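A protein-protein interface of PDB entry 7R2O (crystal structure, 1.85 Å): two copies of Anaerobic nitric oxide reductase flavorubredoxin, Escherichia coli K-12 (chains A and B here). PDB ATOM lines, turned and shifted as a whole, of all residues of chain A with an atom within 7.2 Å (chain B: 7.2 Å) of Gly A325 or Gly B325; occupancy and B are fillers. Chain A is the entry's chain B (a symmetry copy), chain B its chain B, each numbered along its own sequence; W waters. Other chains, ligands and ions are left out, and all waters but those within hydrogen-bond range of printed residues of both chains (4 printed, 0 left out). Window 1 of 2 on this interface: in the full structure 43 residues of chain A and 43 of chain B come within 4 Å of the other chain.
Water W1 bridges OE2 of Glu A26 (2.7 Å) and N of Lys B322 (2.9 Å).
Water W4 bridges OE2 of Glu B26 (2.7 Å) and N of Lys A322 (2.9 Å).
Water W3 lies within hydrogen-bond range of the side-chain carboxylate (OE1) of Glu B328 (2.9 Å) and the guanidinium group (NH2) of Arg A359 (3.0 Å).
Water W2 bridges the side-chain carboxylate of Glu A328 (2.9 Å) and the guanidinium group of Arg B359 (3.0 Å).
The side-chain amino group of Lys A295 is in salt-bridge range of the side-chain carboxylate of Glu A329.
The side-chain carboxylate (OE1) of Glu A26 lies within salt-bridge range of the side-chain amino group (NZ) of Lys A295 (2.8 Å).
The side-chain carboxylate of Glu B329 lies within salt-bridge range of the side-chain amino group of Lys B295.
NZ of Lys B295 lies within salt-bridge range of OE1 of Glu B26 (2.8 Å).
Hydrophobic or aromatic side chains of chain A that line the printed part of chain B: Met A319, Met A320, Pro A321 and Ala A324.
Among the printed residues, 17 pairs touch across the chains.
Among the printed residues, Asp or Glu carboxylates within 4 Å of a Lys or Arg side-chain nitrogen of the other chain: Glu A26 with Lys B322 (2.7 Å), Lys A322 with Glu B26 (2.7 Å), Glu A328 with Arg B359 (3.2 Å) and Arg A359 with Glu B328 (3.2 Å).
The side-chain carboxylate of Glu A328 lies close to the backbone NH of Met B319, 3.2 Å away.
The backbone NH (N) of Met A319 lies close to the side-chain carboxylate (OE2) of Glu B328 (3.2 Å).
NZ of Lys A322 lies within salt-bridge range of OE2 of Glu B26 (2.7 Å).
The side-chain carboxylate (OE1) of Glu A328 is in salt-bridge range of the guanidinium group (NH1) of Arg B359, 3.2 Å away.
NZ of Lys B322 lies within salt-bridge range of OE2 of Glu A26.
The side-chain carboxylate (OE1) of Glu B328 lies within salt-bridge range of the guanidinium group (NH1) of Arg A359.
Of the printed residues of chain B, Gly A325 touches Pro B321 (3.2 Å) and Gly B325 (3.9 Å).
Of the printed residues of chain A, Gly B325 touches Pro A321 and Gly A325.
Ala B324 touches one residue of chain A.
Printed residues of chain A within 4 Å of Lys B322: Glu A26.
Printed residues of chain B within 4 Å of Glu A329: Pro B321.
Of the printed residues of chain A, Met B320 touches Glu A26.
Of the printed residues of chain B, Lys A322 touches Glu B26 (2.7 Å).
Leu A326 touches none of the printed residues of chain B.
The nearest residue of chain B that does not touch Gly A325 is Ala B324 (4.2 Å).
The nearest residue of chain A that does not touch Gly B325 is Ala A324 (4.2 Å).
The nearest printed residue of chain A that does not touch Lys B322 is Gly A325 (5.1 Å).
Pro A321 touches Glu B329, and with the chains exchanged Glu A329 touches Pro B321.
Ala A324 touches Glu B328, and with the chains exchanged Glu A328 touches Ala B324.
Gly A325 touches its own counterpart, Gly B325.
Glu A328 touches Arg B359, and with the chains exchanged Arg A359 touches Glu B328.
16 positions are printed for both chains.
Among the printed residues, merely in contact across the chains: Pro A321 with Gly B325 (3.2 Å), Gly A325 with Pro B321 (3.2 Å), Pro A321 with Glu B26 (3.3 Å), Glu A26 with Pro B321 (3.3 Å), Glu A26 with Met B320 (3.3 Å), Met A320 with Glu B26 (3.3 Å), Glu A328 with Ala B324 (3.5 Å), Ala A324 with Glu B328 (3.5 Å), Pro A321 with Glu B329 (3.7 Å), Glu A329 with Pro B321 (3.7 Å) and Gly A325 with Gly B325 (3.9 Å).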
ATOM      1  N   GLU A  26      -9.224 -21.329 -30.019  1.00  0.00           N
ATOM      2  CA  GLU A  26      -8.199 -20.359 -30.370  1.00  0.00           C
ATOM      3  C   GLU A  26      -8.749 -18.951 -30.559  1.00  0.00           C
ATOM      4  O   GLU A  26      -7.965 -18.020 -30.779  1.00  0.00           O
ATOM      5  CB  GLU A  26      -7.454 -20.805 -31.633  1.00  0.00           C
ATOM      6  CG  GLU A  26      -6.738 -22.145 -31.483  1.00  0.00           C
ATOM      7  CD  GLU A  26      -5.888 -22.228 -30.223  1.00  0.00           C
ATOM      8  OE1 GLU A  26      -5.310 -21.196 -29.822  1.00  0.00           O
ATOM      9  OE2 GLU A  26      -5.806 -23.327 -29.628  1.00  0.00           O
ATOM     10  N   LYS A 295      -5.305 -15.073 -24.583  1.00  0.00           N
ATOM     11  CA  LYS A 295      -4.352 -15.088 -25.689  1.00  0.00           C
ATOM     12  C   LYS A 295      -4.772 -14.137 -26.801  1.00  0.00           C
ATOM     13  O   LYS A 295      -3.926 -13.483 -27.423  1.00  0.00           O
ATOM     14  CB  LYS A 295      -4.214 -16.509 -26.234  1.00  0.00           C
ATOM     15  CG  LYS A 295      -3.307 -16.622 -27.437  1.00  0.00           C
ATOM     16  CD  LYS A 295      -3.722 -17.776 -28.331  1.00  0.00           C
ATOM     17  CE  LYS A 295      -5.062 -17.506 -28.991  1.00  0.00           C
ATOM     18  NZ  LYS A 295      -5.328 -18.447 -30.116  1.00  0.00           N
ATOM     19  N   MET A 319      12.070 -23.911 -24.951  1.00  0.00           N
ATOM     20  CA  MET A 319      11.261 -22.851 -24.380  1.00  0.00           C
ATOM     21  C   MET A 319       9.985 -23.438 -23.785  1.00  0.00           C
ATOM     22  O   MET A 319       9.626 -24.593 -24.024  1.00  0.00           O
ATOM     23  CB  MET A 319      10.949 -21.781 -25.430  1.00  0.00           C
ATOM     24  CG  MET A 319      10.149 -22.254 -26.626  1.00  0.00           C
ATOM     25  SD  MET A 319      10.136 -21.021 -27.951  1.00  0.00           S
ATOM     26  CE  MET A 319      11.728 -21.308 -28.709  1.00  0.00           C
ATOM     27  N   MET A 320       9.309 -22.636 -22.978  1.00  0.00           N
ATOM     28  CA  MET A 320       8.092 -23.118 -22.356  1.00  0.00           C
ATOM     29  C   MET A 320       7.006 -23.289 -23.417  1.00  0.00           C
ATOM     30  O   MET A 320       6.885 -22.457 -24.323  1.00  0.00           O
ATOM     31  CB  MET A 320       7.645 -22.167 -21.254  1.00  0.00           C
ATOM     32  CG  MET A 320       8.661 -22.123 -20.122  1.00  0.00           C
ATOM     33  SD  MET A 320       7.946 -21.702 -18.539  1.00  0.00           S
ATOM     34  CE  MET A 320       6.801 -23.054 -18.301  1.00  0.00           C
ATOM     35  N   PRO A 321       6.218 -24.364 -23.336  1.00  0.00           N
ATOM     36  CA  PRO A 321       5.362 -24.735 -24.478  1.00  0.00           C
ATOM     37  C   PRO A 321       4.361 -23.668 -24.889  1.00  0.00           C
ATOM     38  O   PRO A 321       4.095 -23.515 -26.087  1.00  0.00           O
ATOM     39  CB  PRO A 321       4.667 -26.017 -23.989  1.00  0.00           C
ATOM     40  CG  PRO A 321       4.880 -26.051 -22.501  1.00  0.00           C
ATOM     41  CD  PRO A 321       6.183 -25.368 -22.260  1.00  0.00           C
ATOM     42  N   LYS A 322       3.789 -22.926 -23.940  1.00  0.00           N
ATOM     43  CA  LYS A 322       2.829 -21.894 -24.318  1.00  0.00           C
ATOM     44  C   LYS A 322       3.486 -20.794 -25.147  1.00  0.00           C
ATOM     45  O   LYS A 322       2.838 -20.205 -26.022  1.00  0.00           O
ATOM     46  CB  LYS A 322       2.168 -21.305 -23.073  1.00  0.00           C
ATOM     47  CG  LYS A 322       1.224 -22.257 -22.373  1.00  0.00           C
ATOM     48  CD  LYS A 322       0.568 -21.590 -21.185  1.00  0.00           C
ATOM     49  CE  LYS A 322      -0.337 -22.564 -20.459  1.00  0.00           C
ATOM     50  NZ  LYS A 322       0.414 -23.777 -20.023  1.00  0.00           N
ATOM     51  N   ILE A 323       4.764 -20.502 -24.888  1.00  0.00           N
ATOM     52  CA  ILE A 323       5.484 -19.543 -25.722  1.00  0.00           C
ATOM     53  C   ILE A 323       5.724 -20.123 -27.113  1.00  0.00           C
ATOM     54  O   ILE A 323       5.513 -19.450 -28.130  1.00  0.00           O
ATOM     55  CB  ILE A 323       6.802 -19.125 -25.040  1.00  0.00           C
ATOM     56  CG1 ILE A 323       6.508 -18.396 -23.729  1.00  0.00           C
ATOM     57  CG2 ILE A 323       7.644 -18.258 -25.970  1.00  0.00           C
ATOM     58  CD1 ILE A 323       5.707 -17.119 -23.902  1.00  0.00           C
ATOM     59  N   ALA A 324       6.165 -21.378 -27.183  1.00  0.00           N
ATOM     60  CA  ALA A 324       6.304 -22.031 -28.480  1.00  0.00           C
ATOM     61  C   ALA A 324       4.992 -21.984 -29.258  1.00  0.00           C
ATOM     62  O   ALA A 324       4.967 -21.621 -30.442  1.00  0.00           O
ATOM     63  CB  ALA A 324       6.774 -23.473 -28.288  1.00  0.00           C
ATOM     64  N   GLY A 325       3.884 -22.332 -28.598  1.00  0.00           N
ATOM     65  CA  GLY A 325       2.599 -22.333 -29.278  1.00  0.00           C
ATOM     66  C   GLY A 325       2.187 -20.954 -29.758  1.00  0.00           C
ATOM     67  O   GLY A 325       1.714 -20.791 -30.887  1.00  0.00           O
ATOM     68  N   LEU A 326       2.363 -19.941 -28.909  1.00  0.00           N
ATOM     69  CA  LEU A 326       1.993 -18.588 -29.304  1.00  0.00           C
ATOM     70  C   LEU A 326       2.887 -18.079 -30.433  1.00  0.00           C
ATOM     71  O   LEU A 326       2.414 -17.387 -31.344  1.00  0.00           O
ATOM     72  CB  LEU A 326       2.049 -17.662 -28.090  1.00  0.00           C
ATOM     73  CG  LEU A 326       1.420 -16.273 -28.209  1.00  0.00           C
ATOM     74  CD1 LEU A 326       0.038 -16.328 -28.850  1.00  0.00           C
ATOM     75  CD2 LEU A 326       1.345 -15.638 -26.831  1.00  0.00           C
ATOM     76  N   VAL A 327       4.175 -18.424 -30.402  1.00  0.00           N
ATOM     77  CA  VAL A 327       5.060 -18.025 -31.493  1.00  0.00           C
ATOM     78  C   VAL A 327       4.674 -18.739 -32.782  1.00  0.00           C
ATOM     79  O   VAL A 327       4.723 -18.151 -33.869  1.00  0.00           O
ATOM     80  CB  VAL A 327       6.533 -18.275 -31.122  1.00  0.00           C
ATOM     81  CG1 VAL A 327       7.423 -18.104 -32.345  1.00  0.00           C
ATOM     82  CG2 VAL A 327       6.963 -17.320 -30.022  1.00  0.00           C
ATOM     83  N   GLU A 328       4.284 -20.015 -32.691  1.00  0.00           N
ATOM     84  CA  GLU A 328       3.756 -20.695 -33.868  1.00  0.00           C
ATOM     85  C   GLU A 328       2.575 -19.922 -34.446  1.00  0.00           C
ATOM     86  O   GLU A 328       2.496 -19.698 -35.659  1.00  0.00           O
ATOM     87  CB  GLU A 328       3.351 -22.130 -33.521  1.00  0.00           C
ATOM     88  CG  GLU A 328       2.688 -22.920 -34.669  1.00  0.00           C
ATOM     89  CD  GLU A 328       3.675 -23.447 -35.715  1.00  0.00           C
ATOM     90  OE1 GLU A 328       4.867 -23.080 -35.662  1.00  0.00           O
ATOM     91  OE2 GLU A 328       3.254 -24.232 -36.595  1.00  0.00           O
ATOM     92  N   GLU A 329       1.652 -19.484 -33.585  1.00  0.00           N
ATOM     93  CA  GLU A 329       0.466 -18.805 -34.094  1.00  0.00           C
ATOM     94  C   GLU A 329       0.826 -17.476 -34.740  1.00  0.00           C
ATOM     95  O   GLU A 329       0.273 -17.120 -35.790  1.00  0.00           O
ATOM     96  CB  GLU A 329      -0.559 -18.592 -32.982  1.00  0.00           C
ATOM     97  CG  GLU A 329      -1.799 -17.856 -33.476  1.00  0.00           C
ATOM     98  CD  GLU A 329      -2.985 -18.010 -32.557  1.00  0.00           C
ATOM     99  OE1 GLU A 329      -2.787 -18.400 -31.388  1.00  0.00           O
ATOM    100  OE2 GLU A 329      -4.120 -17.746 -33.007  1.00  0.00           O
ATOM    101  N   MET A 330       1.747 -16.727 -34.129  1.00  0.00           N
ATOM    102  CA  MET A 330       2.173 -15.467 -34.727  1.00  0.00           C
ATOM    103  C   MET A 330       2.819 -15.687 -36.085  1.00  0.00           C
ATOM    104  O   MET A 330       2.686 -14.844 -36.977  1.00  0.00           O
ATOM    105  CB  MET A 330       3.134 -14.736 -33.794  1.00  0.00           C
ATOM    106  CG  MET A 330       2.475 -14.203 -32.543  1.00  0.00           C
ATOM    107  SD  MET A 330       3.494 -12.968 -31.727  1.00  0.00           S
ATOM    108  CE  MET A 330       4.888 -13.975 -31.210  1.00  0.00           C
ATOM    109  N   THR A 331       3.521 -16.807 -36.263  1.00  0.00           N
ATOM    110  CA  THR A 331       4.119 -17.099 -37.562  1.00  0.00           C
ATOM    111  C   THR A 331       3.056 -17.153 -38.652  1.00  0.00           C
ATOM    112  O   THR A 331       3.302 -16.741 -39.790  1.00  0.00           O
ATOM    113  CB  THR A 331       4.899 -18.415 -37.503  1.00  0.00           C
ATOM    114  OG1 THR A 331       5.921 -18.328 -36.502  1.00  0.00           O
ATOM    115  CG2 THR A 331       5.550 -18.706 -38.846  1.00  0.00           C
ATOM    116  N   ARG A 359      13.043 -18.126 -33.515  1.00  0.00           N
ATOM    117  CA  ARG A 359      11.679 -18.361 -33.982  1.00  0.00           C
ATOM    118  C   ARG A 359      10.884 -17.065 -34.101  1.00  0.00           C
ATOM    119  O   ARG A 359       9.994 -16.966 -34.953  1.00  0.00           O
ATOM    120  CB  ARG A 359      10.971 -19.356 -33.067  1.00  0.00           C
ATOM    121  CG  ARG A 359      11.450 -20.776 -33.272  1.00  0.00           C
ATOM    122  CD  ARG A 359      10.604 -21.786 -32.527  1.00  0.00           C
ATOM    123  NE  ARG A 359      11.141 -23.135 -32.677  1.00  0.00           N
ATOM    124  CZ  ARG A 359      10.547 -24.231 -32.221  1.00  0.00           C
ATOM    125  NH1 ARG A 359       9.388 -24.141 -31.584  1.00  0.00           N
ATOM    126  NH2 ARG A 359      11.111 -25.417 -32.404  1.00  0.00           N
ATOM    127  N   GLU B  26       2.819 -26.001 -15.964  1.00  0.00           N
ATOM    128  CA  GLU B  26       3.182 -27.101 -16.844  1.00  0.00           C
ATOM    129  C   GLU B  26       3.160 -28.455 -16.148  1.00  0.00           C
ATOM    130  O   GLU B  26       3.369 -29.478 -16.809  1.00  0.00           O
ATOM    131  CB  GLU B  26       4.560 -26.852 -17.466  1.00  0.00           C
ATOM    132  CG  GLU B  26       4.632 -25.586 -18.316  1.00  0.00           C
ATOM    133  CD  GLU B  26       3.491 -25.476 -19.318  1.00  0.00           C
ATOM    134  OE1 GLU B  26       3.053 -26.521 -19.843  1.00  0.00           O
ATOM    135  OE2 GLU B  26       3.026 -24.341 -19.574  1.00  0.00           O
ATOM    136  N   LYS B 295      -2.759 -32.102 -19.926  1.00  0.00           N
ATOM    137  CA  LYS B 295      -1.557 -32.288 -20.734  1.00  0.00           C
ATOM    138  C   LYS B 295      -0.605 -33.289 -20.095  1.00  0.00           C
ATOM    139  O   LYS B 295       0.038 -34.082 -20.794  1.00  0.00           O
ATOM    140  CB  LYS B 295      -0.855 -30.946 -20.934  1.00  0.00           C
ATOM    141  CG  LYS B 295       0.447 -31.039 -21.693  1.00  0.00           C
ATOM    142  CD  LYS B 295       1.404 -29.935 -21.280  1.00  0.00           C
ATOM    143  CE  LYS B 295       1.877 -30.125 -19.850  1.00  0.00           C
ATOM    144  NZ  LYS B 295       3.056 -29.268 -19.536  1.00  0.00           N
ATOM    145  N   MET B 319       0.485 -25.188 -37.865  1.00  0.00           N
ATOM    146  CA  MET B 319      -0.281 -26.101 -37.038  1.00  0.00           C
ATOM    147  C   MET B 319      -0.952 -25.333 -35.904  1.00  0.00           C
ATOM    148  O   MET B 319      -0.637 -24.173 -35.626  1.00  0.00           O
ATOM    149  CB  MET B 319       0.610 -27.225 -36.503  1.00  0.00           C
ATOM    150  CG  MET B 319       1.751 -26.784 -35.609  1.00  0.00           C
ATOM    151  SD  MET B 319       2.931 -28.125 -35.320  1.00  0.00           S
ATOM    152  CE  MET B 319       3.890 -28.076 -36.826  1.00  0.00           C
ATOM    153  N   MET B 320      -1.909 -25.981 -35.262  1.00  0.00           N
ATOM    154  CA  MET B 320      -2.611 -25.321 -34.180  1.00  0.00           C
ATOM    155  C   MET B 320      -1.668 -25.136 -32.992  1.00  0.00           C
ATOM    156  O   MET B 320      -0.872 -26.031 -32.684  1.00  0.00           O
ATOM    157  CB  MET B 320      -3.849 -26.115 -33.785  1.00  0.00           C
ATOM    158  CG  MET B 320      -4.857 -26.159 -34.924  1.00  0.00           C
ATOM    159  SD  MET B 320      -6.546 -26.356 -34.373  1.00  0.00           S
ATOM    160  CE  MET B 320      -6.771 -24.876 -33.395  1.00  0.00           C
ATOM    161  N   PRO B 321      -1.725 -23.982 -32.322  1.00  0.00           N
ATOM    162  CA  PRO B 321      -0.655 -23.631 -31.371  1.00  0.00           C
ATOM    163  C   PRO B 321      -0.473 -24.622 -30.233  1.00  0.00           C
ATOM    164  O   PRO B 321       0.666 -24.856 -29.809  1.00  0.00           O
ATOM    165  CB  PRO B 321      -1.083 -22.245 -30.862  1.00  0.00           C
ATOM    166  CG  PRO B 321      -2.526 -22.096 -31.259  1.00  0.00           C
ATOM    167  CD  PRO B 321      -2.687 -22.886 -32.512  1.00  0.00           C
ATOM    168  N   LYS B 322      -1.552 -25.210 -29.715  1.00  0.00           N
ATOM    169  CA  LYS B 322      -1.394 -26.167 -28.625  1.00  0.00           C
ATOM    170  C   LYS B 322      -0.615 -27.401 -29.071  1.00  0.00           C
ATOM    171  O   LYS B 322       0.116 -27.998 -28.270  1.00  0.00           O
ATOM    172  CB  LYS B 322      -2.760 -26.567 -28.070  1.00  0.00           C
ATOM    173  CG  LYS B 322      -3.459 -25.462 -27.312  1.00  0.00           C
ATOM    174  CD  LYS B 322      -4.777 -25.945 -26.747  1.00  0.00           C
ATOM    175  CE  LYS B 322      -5.495 -24.819 -26.032  1.00  0.00           C
ATOM    176  NZ  LYS B 322      -5.715 -23.656 -26.940  1.00  0.00           N
ATOM    177  N   ILE B 323      -0.756 -27.800 -30.339  1.00  0.00           N
ATOM    178  CA  ILE B 323       0.050 -28.901 -30.860  1.00  0.00           C
ATOM    179  C   ILE B 323       1.511 -28.479 -30.980  1.00  0.00           C
ATOM    180  O   ILE B 323       2.422 -29.218 -30.585  1.00  0.00           O
ATOM    181  CB  ILE B 323      -0.519 -29.389 -32.207  1.00  0.00           C
ATOM    182  CG1 ILE B 323      -1.924 -29.959 -32.011  1.00  0.00           C
ATOM    183  CG2 ILE B 323       0.405 -30.421 -32.846  1.00  0.00           C
ATOM    184  CD1 ILE B 323      -1.975 -31.156 -31.080  1.00  0.00           C
ATOM    185  N   ALA B 324       1.761 -27.288 -31.523  1.00  0.00           N
ATOM    186  CA  ALA B 324       3.125 -26.776 -31.561  1.00  0.00           C
ATOM    187  C   ALA B 324       3.742 -26.758 -30.165  1.00  0.00           C
ATOM    188  O   ALA B 324       4.871 -27.224 -29.962  1.00  0.00           O
ATOM    189  CB  ALA B 324       3.139 -25.379 -32.182  1.00  0.00           C
ATOM    190  N   GLY B 325       3.000 -26.238 -29.183  1.00  0.00           N
ATOM    191  CA  GLY B 325       3.527 -26.166 -27.830  1.00  0.00           C
ATOM    192  C   GLY B 325       3.812 -27.533 -27.237  1.00  0.00           C
ATOM    193  O   GLY B 325       4.857 -27.749 -26.616  1.00  0.00           O
ATOM    194  N   LEU B 326       2.887 -28.476 -27.422  1.00  0.00           N
ATOM    195  CA  LEU B 326       3.095 -29.814 -26.882  1.00  0.00           C
ATOM    196  C   LEU B 326       4.259 -30.515 -27.580  1.00  0.00           C
ATOM    197  O   LEU B 326       5.034 -31.235 -26.938  1.00  0.00           O
ATOM    198  CB  LEU B 326       1.806 -30.625 -27.002  1.00  0.00           C
ATOM    199  CG  LEU B 326       1.708 -31.947 -26.238  1.00  0.00           C
ATOM    200  CD1 LEU B 326       2.191 -31.807 -24.798  1.00  0.00           C
ATOM    201  CD2 LEU B 326       0.272 -32.440 -26.274  1.00  0.00           C
ATOM    202  N   VAL B 327       4.410 -30.305 -28.889  1.00  0.00           N
ATOM    203  CA  VAL B 327       5.546 -30.892 -29.593  1.00  0.00           C
ATOM    204  C   VAL B 327       6.851 -30.263 -29.120  1.00  0.00           C
ATOM    205  O   VAL B 327       7.869 -30.951 -28.981  1.00  0.00           O
ATOM    206  CB  VAL B 327       5.372 -30.763 -31.117  1.00  0.00           C
ATOM    207  CG1 VAL B 327       6.664 -31.138 -31.831  1.00  0.00           C
ATOM    208  CG2 VAL B 327       4.234 -31.652 -31.589  1.00  0.00           C
ATOM    209  N   GLU B 328       6.849 -28.951 -28.863  1.00  0.00           N
ATOM    210  CA  GLU B 328       8.023 -28.331 -28.259  1.00  0.00           C
ATOM    211  C   GLU B 328       8.380 -29.027 -26.951  1.00  0.00           C
ATOM    212  O   GLU B 328       9.548 -29.353 -26.702  1.00  0.00           O
ATOM    213  CB  GLU B 328       7.784 -26.836 -28.034  1.00  0.00           C
ATOM    214  CG  GLU B 328       8.925 -26.091 -27.311  1.00  0.00           C
ATOM    215  CD  GLU B 328      10.125 -25.768 -28.207  1.00  0.00           C
ATOM    216  OE1 GLU B 328      10.169 -26.250 -29.357  1.00  0.00           O
ATOM    217  OE2 GLU B 328      11.028 -25.028 -27.755  1.00  0.00           O
ATOM    218  N   GLU B 329       7.380 -29.286 -26.104  1.00  0.00           N
ATOM    219  CA  GLU B 329       7.679 -29.882 -24.806  1.00  0.00           C
ATOM    220  C   GLU B 329       8.220 -31.296 -24.960  1.00  0.00           C
ATOM    221  O   GLU B 329       9.157 -31.687 -24.253  1.00  0.00           O
ATOM    222  CB  GLU B 329       6.442 -29.884 -23.910  1.00  0.00           C
ATOM    223  CG  GLU B 329       6.714 -30.530 -22.556  1.00  0.00           C
ATOM    224  CD  GLU B 329       5.687 -30.170 -21.511  1.00  0.00           C
ATOM    225  OE1 GLU B 329       4.596 -29.696 -21.886  1.00  0.00           O
ATOM    226  OE2 GLU B 329       5.977 -30.354 -20.310  1.00  0.00           O
ATOM    227  N   MET B 330       7.642 -32.076 -25.877  1.00  0.00           N
ATOM    228  CA  MET B 330       8.150 -33.423 -26.108  1.00  0.00           C
ATOM    229  C   MET B 330       9.588 -33.398 -26.600  1.00  0.00           C
ATOM    230  O   MET B 330      10.367 -34.302 -26.281  1.00  0.00           O
ATOM    231  CB  MET B 330       7.260 -34.162 -27.105  1.00  0.00           C
ATOM    232  CG  MET B 330       5.895 -34.505 -26.557  1.00  0.00           C
ATOM    233  SD  MET B 330       5.076 -35.758 -27.551  1.00  0.00           S
ATOM    234  CE  MET B 330       4.827 -34.859 -29.085  1.00  0.00           C
ATOM    235  N   THR B 331       9.960 -32.378 -27.376  1.00  0.00           N
ATOM    236  CA  THR B 331      11.341 -32.271 -27.834  1.00  0.00           C
ATOM    237  C   THR B 331      12.304 -32.208 -26.655  1.00  0.00           C
ATOM    238  O   THR B 331      13.413 -32.746 -26.720  1.00  0.00           O
ATOM    239  CB  THR B 331      11.508 -31.043 -28.733  1.00  0.00           C
ATOM    240  OG1 THR B 331      10.625 -31.143 -29.857  1.00  0.00           O
ATOM    241  CG2 THR B 331      12.938 -30.947 -29.238  1.00  0.00           C
ATOM    242  N   ARG B 359       8.456 -31.807 -37.243  1.00  0.00           N
ATOM    243  CA  ARG B 359       8.789 -31.477 -35.860  1.00  0.00           C
ATOM    244  C   ARG B 359       8.682 -32.688 -34.940  1.00  0.00           C
ATOM    245  O   ARG B 359       9.412 -32.772 -33.946  1.00  0.00           O
ATOM    246  CB  ARG B 359       7.907 -30.333 -35.364  1.00  0.00           C
ATOM    247  CG  ARG B 359       8.312 -28.995 -35.943  1.00  0.00           C
ATOM    248  CD  ARG B 359       7.585 -27.839 -35.291  1.00  0.00           C
ATOM    249  NE  ARG B 359       7.934 -26.572 -35.928  1.00  0.00           N
ATOM    250  CZ  ARG B 359       7.530 -25.383 -35.498  1.00  0.00           C
ATOM    251  NH1 ARG B 359       6.760 -25.292 -34.422  1.00  0.00           N
ATOM    252  NH2 ARG B 359       7.898 -24.283 -36.142  1.00  0.00           N
HETATM  253  O   HOH W   1      -4.286 -25.306 -30.661  1.00  0.00           O
HETATM  254  O   HOH W   2       7.243 -21.768 -34.613  1.00  0.00           O
HETATM  255  O   HOH W   3       9.265 -27.699 -31.713  1.00  0.00           O
HETATM  256  O   HOH W   4       4.424 -22.634 -21.132  1.00  0.00           O
